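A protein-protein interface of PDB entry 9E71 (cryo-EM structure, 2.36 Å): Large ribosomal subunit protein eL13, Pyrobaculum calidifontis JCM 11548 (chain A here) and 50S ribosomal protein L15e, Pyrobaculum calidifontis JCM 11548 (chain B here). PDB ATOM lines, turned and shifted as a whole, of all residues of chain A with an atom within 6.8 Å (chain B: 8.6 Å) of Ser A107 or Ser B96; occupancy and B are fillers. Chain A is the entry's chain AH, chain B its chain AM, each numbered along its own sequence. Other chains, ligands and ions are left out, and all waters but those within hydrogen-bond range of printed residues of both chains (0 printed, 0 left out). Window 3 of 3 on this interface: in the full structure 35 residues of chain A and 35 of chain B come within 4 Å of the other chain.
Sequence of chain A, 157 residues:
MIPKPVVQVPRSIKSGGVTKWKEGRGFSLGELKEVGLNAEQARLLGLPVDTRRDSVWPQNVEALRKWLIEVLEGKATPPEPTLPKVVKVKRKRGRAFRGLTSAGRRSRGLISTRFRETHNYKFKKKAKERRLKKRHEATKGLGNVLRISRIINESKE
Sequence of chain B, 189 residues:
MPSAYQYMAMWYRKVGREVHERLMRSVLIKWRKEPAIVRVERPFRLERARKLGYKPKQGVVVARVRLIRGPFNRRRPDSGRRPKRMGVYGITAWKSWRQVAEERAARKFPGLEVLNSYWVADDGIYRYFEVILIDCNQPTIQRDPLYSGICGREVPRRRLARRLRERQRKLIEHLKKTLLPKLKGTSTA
Of the printed residues of chain B, Ser A107 touches Trp B94 (2.8 Å) and Ser B96 (3.9 Å).
Of chain A, only Ala A103 (3.96 Å) and Ser A107 (3.9 Å) come within 4 Å of Ser B96.
Of the printed residues of chain A, Gln B99 touches Ala A103 (3.9 Å) and Gly A104 (3.8 Å).
Of the printed residues of chain B, Ala A103 touches Ser B96, Arg B98 and Gln B99.
Printed residues of chain B within 4 Å of Gly A104: Gln B99.
Of the printed residues of chain A, Trp B94 touches Ser A107 (2.8 Å).
The nearest printed residue of chain B that does not touch Ala A103 is Glu B102 (4.2 Å).
Ser B96 touches Ala A103.
Arg B98 touches Ala A103.
N of Gln B99 touches CB of Ala A103, 3.9 Å away.
OE1 of Gln B99 touches CA of Gly A104, 3.8 Å away.
Ser B96 touches Ser A107 (N to OG, 3.9 Å).
Printed residues of chain B that touch a printed residue of chain A: Trp B94, Ser B96, Arg B98 and Gln B99.
Hydrophobic or aromatic side chains of chain A that line the printed part of chain B: Ala A103.
Among the printed residues, 6 pairs touch across the chains.
Among the printed residues, no Asp or Glu carboxylate lies within 4 Å of a Lys or Arg side-chain nitrogen of the other chain.
The side-chain hydroxyl (OG) of Ser A107 is in hydrogen-bond range of the backbone carbonyl oxygen (O) of Trp B94 (2.8 Å).
NH1 of Arg B98 lies within hydrogen-bond range of O of Ser B117, at 2.9 Å.
The side-chain amide nitrogen (NE2) of Gln B99 is in hydrogen-bond range of the side-chain carboxylate (OE2) of Glu B103 (3.3 Å).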
ATOM      1  N   SER A 102       7.607  19.319  34.819  1.00  0.00           N
ATOM      2  CA  SER A 102       6.676  20.395  34.493  1.00  0.00           C
ATOM      3  C   SER A 102       5.608  19.936  33.505  1.00  0.00           C
ATOM      4  O   SER A 102       4.430  20.284  33.650  1.00  0.00           O
ATOM      5  CB  SER A 102       7.445  21.590  33.940  1.00  0.00           C
ATOM      6  OG  SER A 102       6.961  22.801  34.484  1.00  0.00           O
ATOM      7  N   ALA A 103       6.000  19.153  32.496  1.00  0.00           N
ATOM      8  CA  ALA A 103       5.032  18.647  31.529  1.00  0.00           C
ATOM      9  C   ALA A 103       4.029  17.711  32.188  1.00  0.00           C
ATOM     10  O   ALA A 103       2.829  17.771  31.899  1.00  0.00           O
ATOM     11  CB  ALA A 103       5.754  17.937  30.386  1.00  0.00           C
ATOM     12  N   GLY A 104       4.508  16.843  33.080  1.00  0.00           N
ATOM     13  CA  GLY A 104       3.606  15.963  33.801  1.00  0.00           C
ATOM     14  C   GLY A 104       2.646  16.718  34.697  1.00  0.00           C
ATOM     15  O   GLY A 104       1.468  16.372  34.786  1.00  0.00           O
ATOM     16  N   ARG A 105       3.137  17.760  35.372  1.00  0.00           N
ATOM     17  CA  ARG A 105       2.265  18.576  36.209  1.00  0.00           C
ATOM     18  C   ARG A 105       1.205  19.282  35.378  1.00  0.00           C
ATOM     19  O   ARG A 105       0.036  19.350  35.778  1.00  0.00           O
ATOM     20  CB  ARG A 105       3.090  19.595  36.992  1.00  0.00           C
ATOM     21  CG  ARG A 105       3.772  19.026  38.215  1.00  0.00           C
ATOM     22  CD  ARG A 105       4.610  20.078  38.910  1.00  0.00           C
ATOM     23  NE  ARG A 105       3.853  21.297  39.155  1.00  0.00           N
ATOM     24  CZ  ARG A 105       3.086  21.491  40.218  1.00  0.00           C
ATOM     25  NH1 ARG A 105       2.951  20.562  41.148  1.00  0.00           N
ATOM     26  NH2 ARG A 105       2.438  22.644  40.349  1.00  0.00           N
ATOM     27  N   ARG A 106       1.593  19.808  34.214  1.00  0.00           N
ATOM     28  CA  ARG A 106       0.627  20.468  33.344  1.00  0.00           C
ATOM     29  C   ARG A 106      -0.430  19.492  32.852  1.00  0.00           C
ATOM     30  O   ARG A 106      -1.622  19.809  32.842  1.00  0.00           O
ATOM     31  CB  ARG A 106       1.336  21.131  32.167  1.00  0.00           C
ATOM     32  CG  ARG A 106       0.380  21.738  31.161  1.00  0.00           C
ATOM     33  CD  ARG A 106       1.098  22.271  29.941  1.00  0.00           C
ATOM     34  NE  ARG A 106       1.863  23.474  30.242  1.00  0.00           N
ATOM     35  CZ  ARG A 106       1.329  24.656  30.507  1.00  0.00           C
ATOM     36  NH1 ARG A 106       0.020  24.837  30.513  1.00  0.00           N
ATOM     37  NH2 ARG A 106       2.128  25.684  30.778  1.00  0.00           N
ATOM     38  N   SER A 107      -0.017  18.287  32.455  1.00  0.00           N
ATOM     39  CA  SER A 107      -0.990  17.297  32.003  1.00  0.00           C
ATOM     40  C   SER A 107      -1.888  16.820  33.136  1.00  0.00           C
ATOM     41  O   SER A 107      -3.053  16.494  32.902  1.00  0.00           O
ATOM     42  CB  SER A 107      -0.286  16.109  31.363  1.00  0.00           C
ATOM     43  OG  SER A 107      -0.413  16.155  29.960  1.00  0.00           O
ATOM     44  N   ARG A 108      -1.370  16.765  34.362  1.00  0.00           N
ATOM     45  CA  ARG A 108      -2.196  16.420  35.508  1.00  0.00           C
ATOM     46  C   ARG A 108      -3.058  17.579  35.977  1.00  0.00           C
ATOM     47  O   ARG A 108      -3.919  17.377  36.836  1.00  0.00           O
ATOM     48  CB  ARG A 108      -1.329  15.932  36.663  1.00  0.00           C
ATOM     49  CG  ARG A 108      -0.572  14.663  36.363  1.00  0.00           C
ATOM     50  CD  ARG A 108       0.549  14.474  37.348  1.00  0.00           C
ATOM     51  NE  ARG A 108       0.042  14.244  38.691  1.00  0.00           N
ATOM     52  CZ  ARG A 108       0.697  14.555  39.798  1.00  0.00           C
ATOM     53  NH1 ARG A 108       1.891  15.117  39.757  1.00  0.00           N
ATOM     54  NH2 ARG A 108       0.137  14.301  40.975  1.00  0.00           N
ATOM     55  N   GLY A 109      -2.840  18.778  35.453  1.00  0.00           N
ATOM     56  CA  GLY A 109      -3.733  19.883  35.712  1.00  0.00           C
ATOM     57  C   GLY A 109      -3.399  20.707  36.929  1.00  0.00           C
ATOM     58  O   GLY A 109      -4.230  21.513  37.357  1.00  0.00           O
ATOM     59  N   LEU A 110      -2.216  20.534  37.497  1.00  0.00           N
ATOM     60  CA  LEU A 110      -1.834  21.272  38.687  1.00  0.00           C
ATOM     61  C   LEU A 110      -1.393  22.696  38.388  1.00  0.00           C
ATOM     62  O   LEU A 110      -1.385  23.527  39.299  1.00  0.00           O
ATOM     63  CB  LEU A 110      -0.730  20.512  39.414  1.00  0.00           C
ATOM     64  CG  LEU A 110      -1.265  19.187  39.947  1.00  0.00           C
ATOM     65  CD1 LEU A 110      -0.172  18.154  40.045  1.00  0.00           C
ATOM     66  CD2 LEU A 110      -1.920  19.410  41.291  1.00  0.00           C
ATOM     67  N   ILE A 111      -1.041  23.001  37.142  1.00  0.00           N
ATOM     68  CA  ILE A 111      -0.699  24.373  36.795  1.00  0.00           C
ATOM     69  C   ILE A 111      -1.937  25.256  36.802  1.00  0.00           C
ATOM     70  O   ILE A 111      -1.892  26.402  37.256  1.00  0.00           O
ATOM     71  CB  ILE A 111       0.020  24.412  35.437  1.00  0.00           C
ATOM     72  CG1 ILE A 111       1.456  23.918  35.588  1.00  0.00           C
ATOM     73  CG2 ILE A 111       0.019  25.816  34.881  1.00  0.00           C
ATOM     74  CD1 ILE A 111       2.251  23.973  34.316  1.00  0.00           C
ATOM     75  N   LEU B  67      10.751  13.482  17.736  1.00  0.00           N
ATOM     76  CA  LEU B  67       9.671  12.503  17.731  1.00  0.00           C
ATOM     77  C   LEU B  67       8.618  12.914  16.719  1.00  0.00           C
ATOM     78  O   LEU B  67       8.642  14.017  16.185  1.00  0.00           O
ATOM     79  CB  LEU B  67       9.050  12.329  19.122  1.00  0.00           C
ATOM     80  CG  LEU B  67       8.557  13.563  19.869  1.00  0.00           C
ATOM     81  CD1 LEU B  67       7.116  13.860  19.514  1.00  0.00           C
ATOM     82  CD2 LEU B  67       8.709  13.349  21.356  1.00  0.00           C
ATOM     83  N   GLY B  70       1.336  14.604  16.009  1.00  0.00           N
ATOM     84  CA  GLY B  70       0.031  14.036  15.789  1.00  0.00           C
ATOM     85  C   GLY B  70      -0.512  13.392  17.044  1.00  0.00           C
ATOM     86  O   GLY B  70       0.154  13.344  18.077  1.00  0.00           O
ATOM     87  N   THR B  92      -6.704  11.109  21.675  1.00  0.00           N
ATOM     88  CA  THR B  92      -5.309  11.342  21.998  1.00  0.00           C
ATOM     89  C   THR B  92      -5.004  10.815  23.392  1.00  0.00           C
ATOM     90  O   THR B  92      -5.890  10.393  24.133  1.00  0.00           O
ATOM     91  CB  THR B  92      -4.969  12.833  21.909  1.00  0.00           C
ATOM     92  OG1 THR B  92      -5.810  13.565  22.805  1.00  0.00           O
ATOM     93  CG2 THR B  92      -5.183  13.343  20.502  1.00  0.00           C
ATOM     94  N   ALA B  93      -3.727  10.846  23.741  1.00  0.00           N
ATOM     95  CA  ALA B  93      -3.282  10.445  25.065  1.00  0.00           C
ATOM     96  C   ALA B  93      -3.294  11.633  26.016  1.00  0.00           C
ATOM     97  O   ALA B  93      -3.209  12.788  25.602  1.00  0.00           O
ATOM     98  CB  ALA B  93      -1.879   9.844  25.004  1.00  0.00           C
ATOM     99  N   TRP B  94      -3.392  11.332  27.306  1.00  0.00           N
ATOM    100  CA  TRP B  94      -3.324  12.362  28.332  1.00  0.00           C
ATOM    101  C   TRP B  94      -1.899  12.788  28.635  1.00  0.00           C
ATOM    102  O   TRP B  94      -1.698  13.713  29.426  1.00  0.00           O
ATOM    103  CB  TRP B  94      -4.002  11.869  29.606  1.00  0.00           C
ATOM    104  CG  TRP B  94      -5.495  11.990  29.582  1.00  0.00           C
ATOM    105  CD1 TRP B  94      -6.292  12.082  28.484  1.00  0.00           C
ATOM    106  CD2 TRP B  94      -6.366  12.042  30.714  1.00  0.00           C
ATOM    107  NE1 TRP B  94      -7.603  12.182  28.859  1.00  0.00           N
ATOM    108  CE2 TRP B  94      -7.677  12.166  30.224  1.00  0.00           C
ATOM    109  CE3 TRP B  94      -6.162  11.996  32.095  1.00  0.00           C
ATOM    110  CZ2 TRP B  94      -8.778  12.234  31.061  1.00  0.00           C
ATOM    111  CZ3 TRP B  94      -7.255  12.069  32.925  1.00  0.00           C
ATOM    112  CH2 TRP B  94      -8.547  12.188  32.407  1.00  0.00           C
ATOM    113  N   LYS B  95      -0.916  12.121  28.051  1.00  0.00           N
ATOM    114  CA  LYS B  95       0.470  12.551  28.099  1.00  0.00           C
ATOM    115  C   LYS B  95       0.752  13.493  26.939  1.00  0.00           C
ATOM    116  O   LYS B  95       0.135  13.401  25.877  1.00  0.00           O
ATOM    117  CB  LYS B  95       1.408  11.349  28.014  1.00  0.00           C
ATOM    118  CG  LYS B  95       2.019  10.929  29.319  1.00  0.00           C
ATOM    119  CD  LYS B  95       2.977   9.777  29.106  1.00  0.00           C
ATOM    120  CE  LYS B  95       3.313   9.103  30.416  1.00  0.00           C
ATOM    121  NZ  LYS B  95       3.942   7.779  30.205  1.00  0.00           N
ATOM    122  N   SER B  96       1.694  14.397  27.146  1.00  0.00           N
ATOM    123  CA  SER B  96       2.132  15.247  26.056  1.00  0.00           C
ATOM    124  C   SER B  96       3.438  14.729  25.469  1.00  0.00           C
ATOM    125  O   SER B  96       4.149  13.914  26.069  1.00  0.00           O
ATOM    126  CB  SER B  96       2.296  16.691  26.519  1.00  0.00           C
ATOM    127  OG  SER B  96       3.322  16.802  27.479  1.00  0.00           O
ATOM    128  N   TRP B  97       3.750  15.222  24.270  1.00  0.00           N
ATOM    129  CA  TRP B  97       4.973  14.803  23.603  1.00  0.00           C
ATOM    130  C   TRP B  97       6.210  15.265  24.354  1.00  0.00           C
ATOM    131  O   TRP B  97       7.263  14.633  24.249  1.00  0.00           O
ATOM    132  CB  TRP B  97       4.997  15.315  22.166  1.00  0.00           C
ATOM    133  CG  TRP B  97       3.986  14.668  21.275  1.00  0.00           C
ATOM    134  CD1 TRP B  97       3.165  15.294  20.391  1.00  0.00           C
ATOM    135  CD2 TRP B  97       3.693  13.270  21.172  1.00  0.00           C
ATOM    136  NE1 TRP B  97       2.375  14.383  19.751  1.00  0.00           N
ATOM    137  CE2 TRP B  97       2.681  13.131  20.211  1.00  0.00           C
ATOM    138  CE3 TRP B  97       4.189  12.122  21.798  1.00  0.00           C
ATOM    139  CZ2 TRP B  97       2.154  11.894  19.861  1.00  0.00           C
ATOM    140  CZ3 TRP B  97       3.661  10.902  21.456  1.00  0.00           C
ATOM    141  CH2 TRP B  97       2.652  10.796  20.496  1.00  0.00           C
ATOM    142  N   ARG B  98       6.106  16.352  25.116  1.00  0.00           N
ATOM    143  CA  ARG B  98       7.221  16.780  25.951  1.00  0.00           C
ATOM    144  C   ARG B  98       7.543  15.735  27.014  1.00  0.00           C
ATOM    145  O   ARG B  98       8.711  15.387  27.228  1.00  0.00           O
ATOM    146  CB  ARG B  98       6.902  18.129  26.588  1.00  0.00           C
ATOM    147  CG  ARG B  98       8.088  18.811  27.231  1.00  0.00           C
ATOM    148  CD  ARG B  98       8.041  20.307  27.019  1.00  0.00           C
ATOM    149  NE  ARG B  98       7.030  20.939  27.856  1.00  0.00           N
ATOM    150  CZ  ARG B  98       7.204  21.251  29.132  1.00  0.00           C
ATOM    151  NH1 ARG B  98       8.335  20.991  29.760  1.00  0.00           N
ATOM    152  NH2 ARG B  98       6.214  21.839  29.796  1.00  0.00           N
ATOM    153  N   GLN B  99       6.516  15.198  27.673  1.00  0.00           N
ATOM    154  CA  GLN B  99       6.760  14.154  28.661  1.00  0.00           C
ATOM    155  C   GLN B  99       7.236  12.870  27.999  1.00  0.00           C
ATOM    156  O   GLN B  99       8.062  12.142  28.565  1.00  0.00           O
ATOM    157  CB  GLN B  99       5.508  13.894  29.490  1.00  0.00           C
ATOM    158  CG  GLN B  99       5.826  13.406  30.890  1.00  0.00           C
ATOM    159  CD  GLN B  99       4.658  12.723  31.561  1.00  0.00           C
ATOM    160  OE1 GLN B  99       3.503  13.079  31.338  1.00  0.00           O
ATOM    161  NE2 GLN B  99       4.953  11.729  32.388  1.00  0.00           N
ATOM    162  N   VAL B 100       6.735  12.582  26.795  1.00  0.00           N
ATOM    163  CA  VAL B 100       7.207  11.418  26.049  1.00  0.00           C
ATOM    164  C   VAL B 100       8.694  11.548  25.729  1.00  0.00           C
ATOM    165  O   VAL B 100       9.465  10.589  25.873  1.00  0.00           O
ATOM    166  CB  VAL B 100       6.363  11.238  24.775  1.00  0.00           C
ATOM    167  CG1 VAL B 100       7.003  10.230  23.844  1.00  0.00           C
ATOM    168  CG2 VAL B 100       4.955  10.812  25.136  1.00  0.00           C
ATOM    169  N   ALA B 101       9.120  12.738  25.306  1.00  0.00           N
ATOM    170  CA  ALA B 101      10.524  12.983  25.004  1.00  0.00           C
ATOM    171  C   ALA B 101      11.388  12.881  26.251  1.00  0.00           C
ATOM    172  O   ALA B 101      12.512  12.364  26.192  1.00  0.00           O
ATOM    173  CB  ALA B 101      10.687  14.355  24.357  1.00  0.00           C
ATOM    174  N   GLU B 102      10.884  13.386  27.381  1.00  0.00           N
ATOM    175  CA  GLU B 102      11.617  13.270  28.640  1.00  0.00           C
ATOM    176  C   GLU B 102      11.831  11.812  29.018  1.00  0.00           C
ATOM    177  O   GLU B 102      12.937  11.411  29.395  1.00  0.00           O
ATOM    178  CB  GLU B 102      10.869  13.998  29.753  1.00  0.00           C
ATOM    179  CG  GLU B 102      10.849  15.499  29.617  1.00  0.00           C
ATOM    180  CD  GLU B 102       9.873  16.150  30.572  1.00  0.00           C
ATOM    181  OE1 GLU B 102       9.046  15.425  31.159  1.00  0.00           O
ATOM    182  OE2 GLU B 102       9.929  17.386  30.738  1.00  0.00           O
ATOM    183  N   GLU B 103      10.782  10.996  28.896  1.00  0.00           N
ATOM    184  CA  GLU B 103      10.906   9.581  29.221  1.00  0.00           C
ATOM    185  C   GLU B 103      11.871   8.871  28.276  1.00  0.00           C
ATOM    186  O   GLU B 103      12.654   8.017  28.707  1.00  0.00           O
ATOM    187  CB  GLU B 103       9.535   8.914  29.184  1.00  0.00           C
ATOM    188  CG  GLU B 103       8.581   9.393  30.259  1.00  0.00           C
ATOM    189  CD  GLU B 103       7.140   9.019  29.966  1.00  0.00           C
ATOM    190  OE1 GLU B 103       6.843   8.640  28.815  1.00  0.00           O
ATOM    191  OE2 GLU B 103       6.305   9.106  30.886  1.00  0.00           O
ATOM    192  N   SER B 117      12.508  20.165  30.337  1.00  0.00           N
ATOM    193  CA  SER B 117      12.648  20.077  28.894  1.00  0.00           C
ATOM    194  C   SER B 117      11.890  21.234  28.268  1.00  0.00           C
ATOM    195  O   SER B 117      11.017  21.836  28.894  1.00  0.00           O
ATOM    196  CB  SER B 117      12.128  18.743  28.360  1.00  0.00           C
ATOM    197  OG  SER B 117      10.851  18.462  28.888  1.00  0.00           O
ATOM    198  N   ARG B 127       8.566  16.827  15.917  1.00  0.00           N
ATOM    199  CA  ARG B 127       8.717  17.847  16.935  1.00  0.00           C
ATOM    200  C   ARG B 127      10.024  17.590  17.664  1.00  0.00           C
ATOM    201  O   ARG B 127      10.408  16.434  17.884  1.00  0.00           O
ATOM    202  CB  ARG B 127       7.551  17.830  17.918  1.00  0.00           C
ATOM    203  CG  ARG B 127       7.620  18.897  18.985  1.00  0.00           C
ATOM    204  CD  ARG B 127       6.233  19.225  19.493  1.00  0.00           C
ATOM    205  NE  ARG B 127       5.406  19.872  18.484  1.00  0.00           N
ATOM    206  CZ  ARG B 127       4.083  19.832  18.469  1.00  0.00           C
ATOM    207  NH1 ARG B 127       3.403  19.162  19.382  1.00  0.00           N
ATOM    208  NH2 ARG B 127       3.425  20.480  17.514  1.00  0.00           N
ATOM    209  N   PHE B 129      12.529  18.507  20.989  1.00  0.00           N
ATOM    210  CA  PHE B 129      12.626  18.979  22.357  1.00  0.00           C
ATOM    211  C   PHE B 129      14.074  18.902  22.806  1.00  0.00           C
ATOM    212  O   PHE B 129      14.882  18.176  22.230  1.00  0.00           O
ATOM    213  CB  PHE B 129      11.752  18.151  23.301  1.00  0.00           C
ATOM    214  CG  PHE B 129      10.292  18.201  22.980  1.00  0.00           C
ATOM    215  CD1 PHE B 129       9.490  19.190  23.511  1.00  0.00           C
ATOM    216  CD2 PHE B 129       9.720  17.250  22.159  1.00  0.00           C
ATOM    217  CE1 PHE B 129       8.152  19.233  23.224  1.00  0.00           C
ATOM    218  CE2 PHE B 129       8.378  17.290  21.871  1.00  0.00           C
ATOM    219  CZ  PHE B 129       7.594  18.281  22.404  1.00  0.00           C
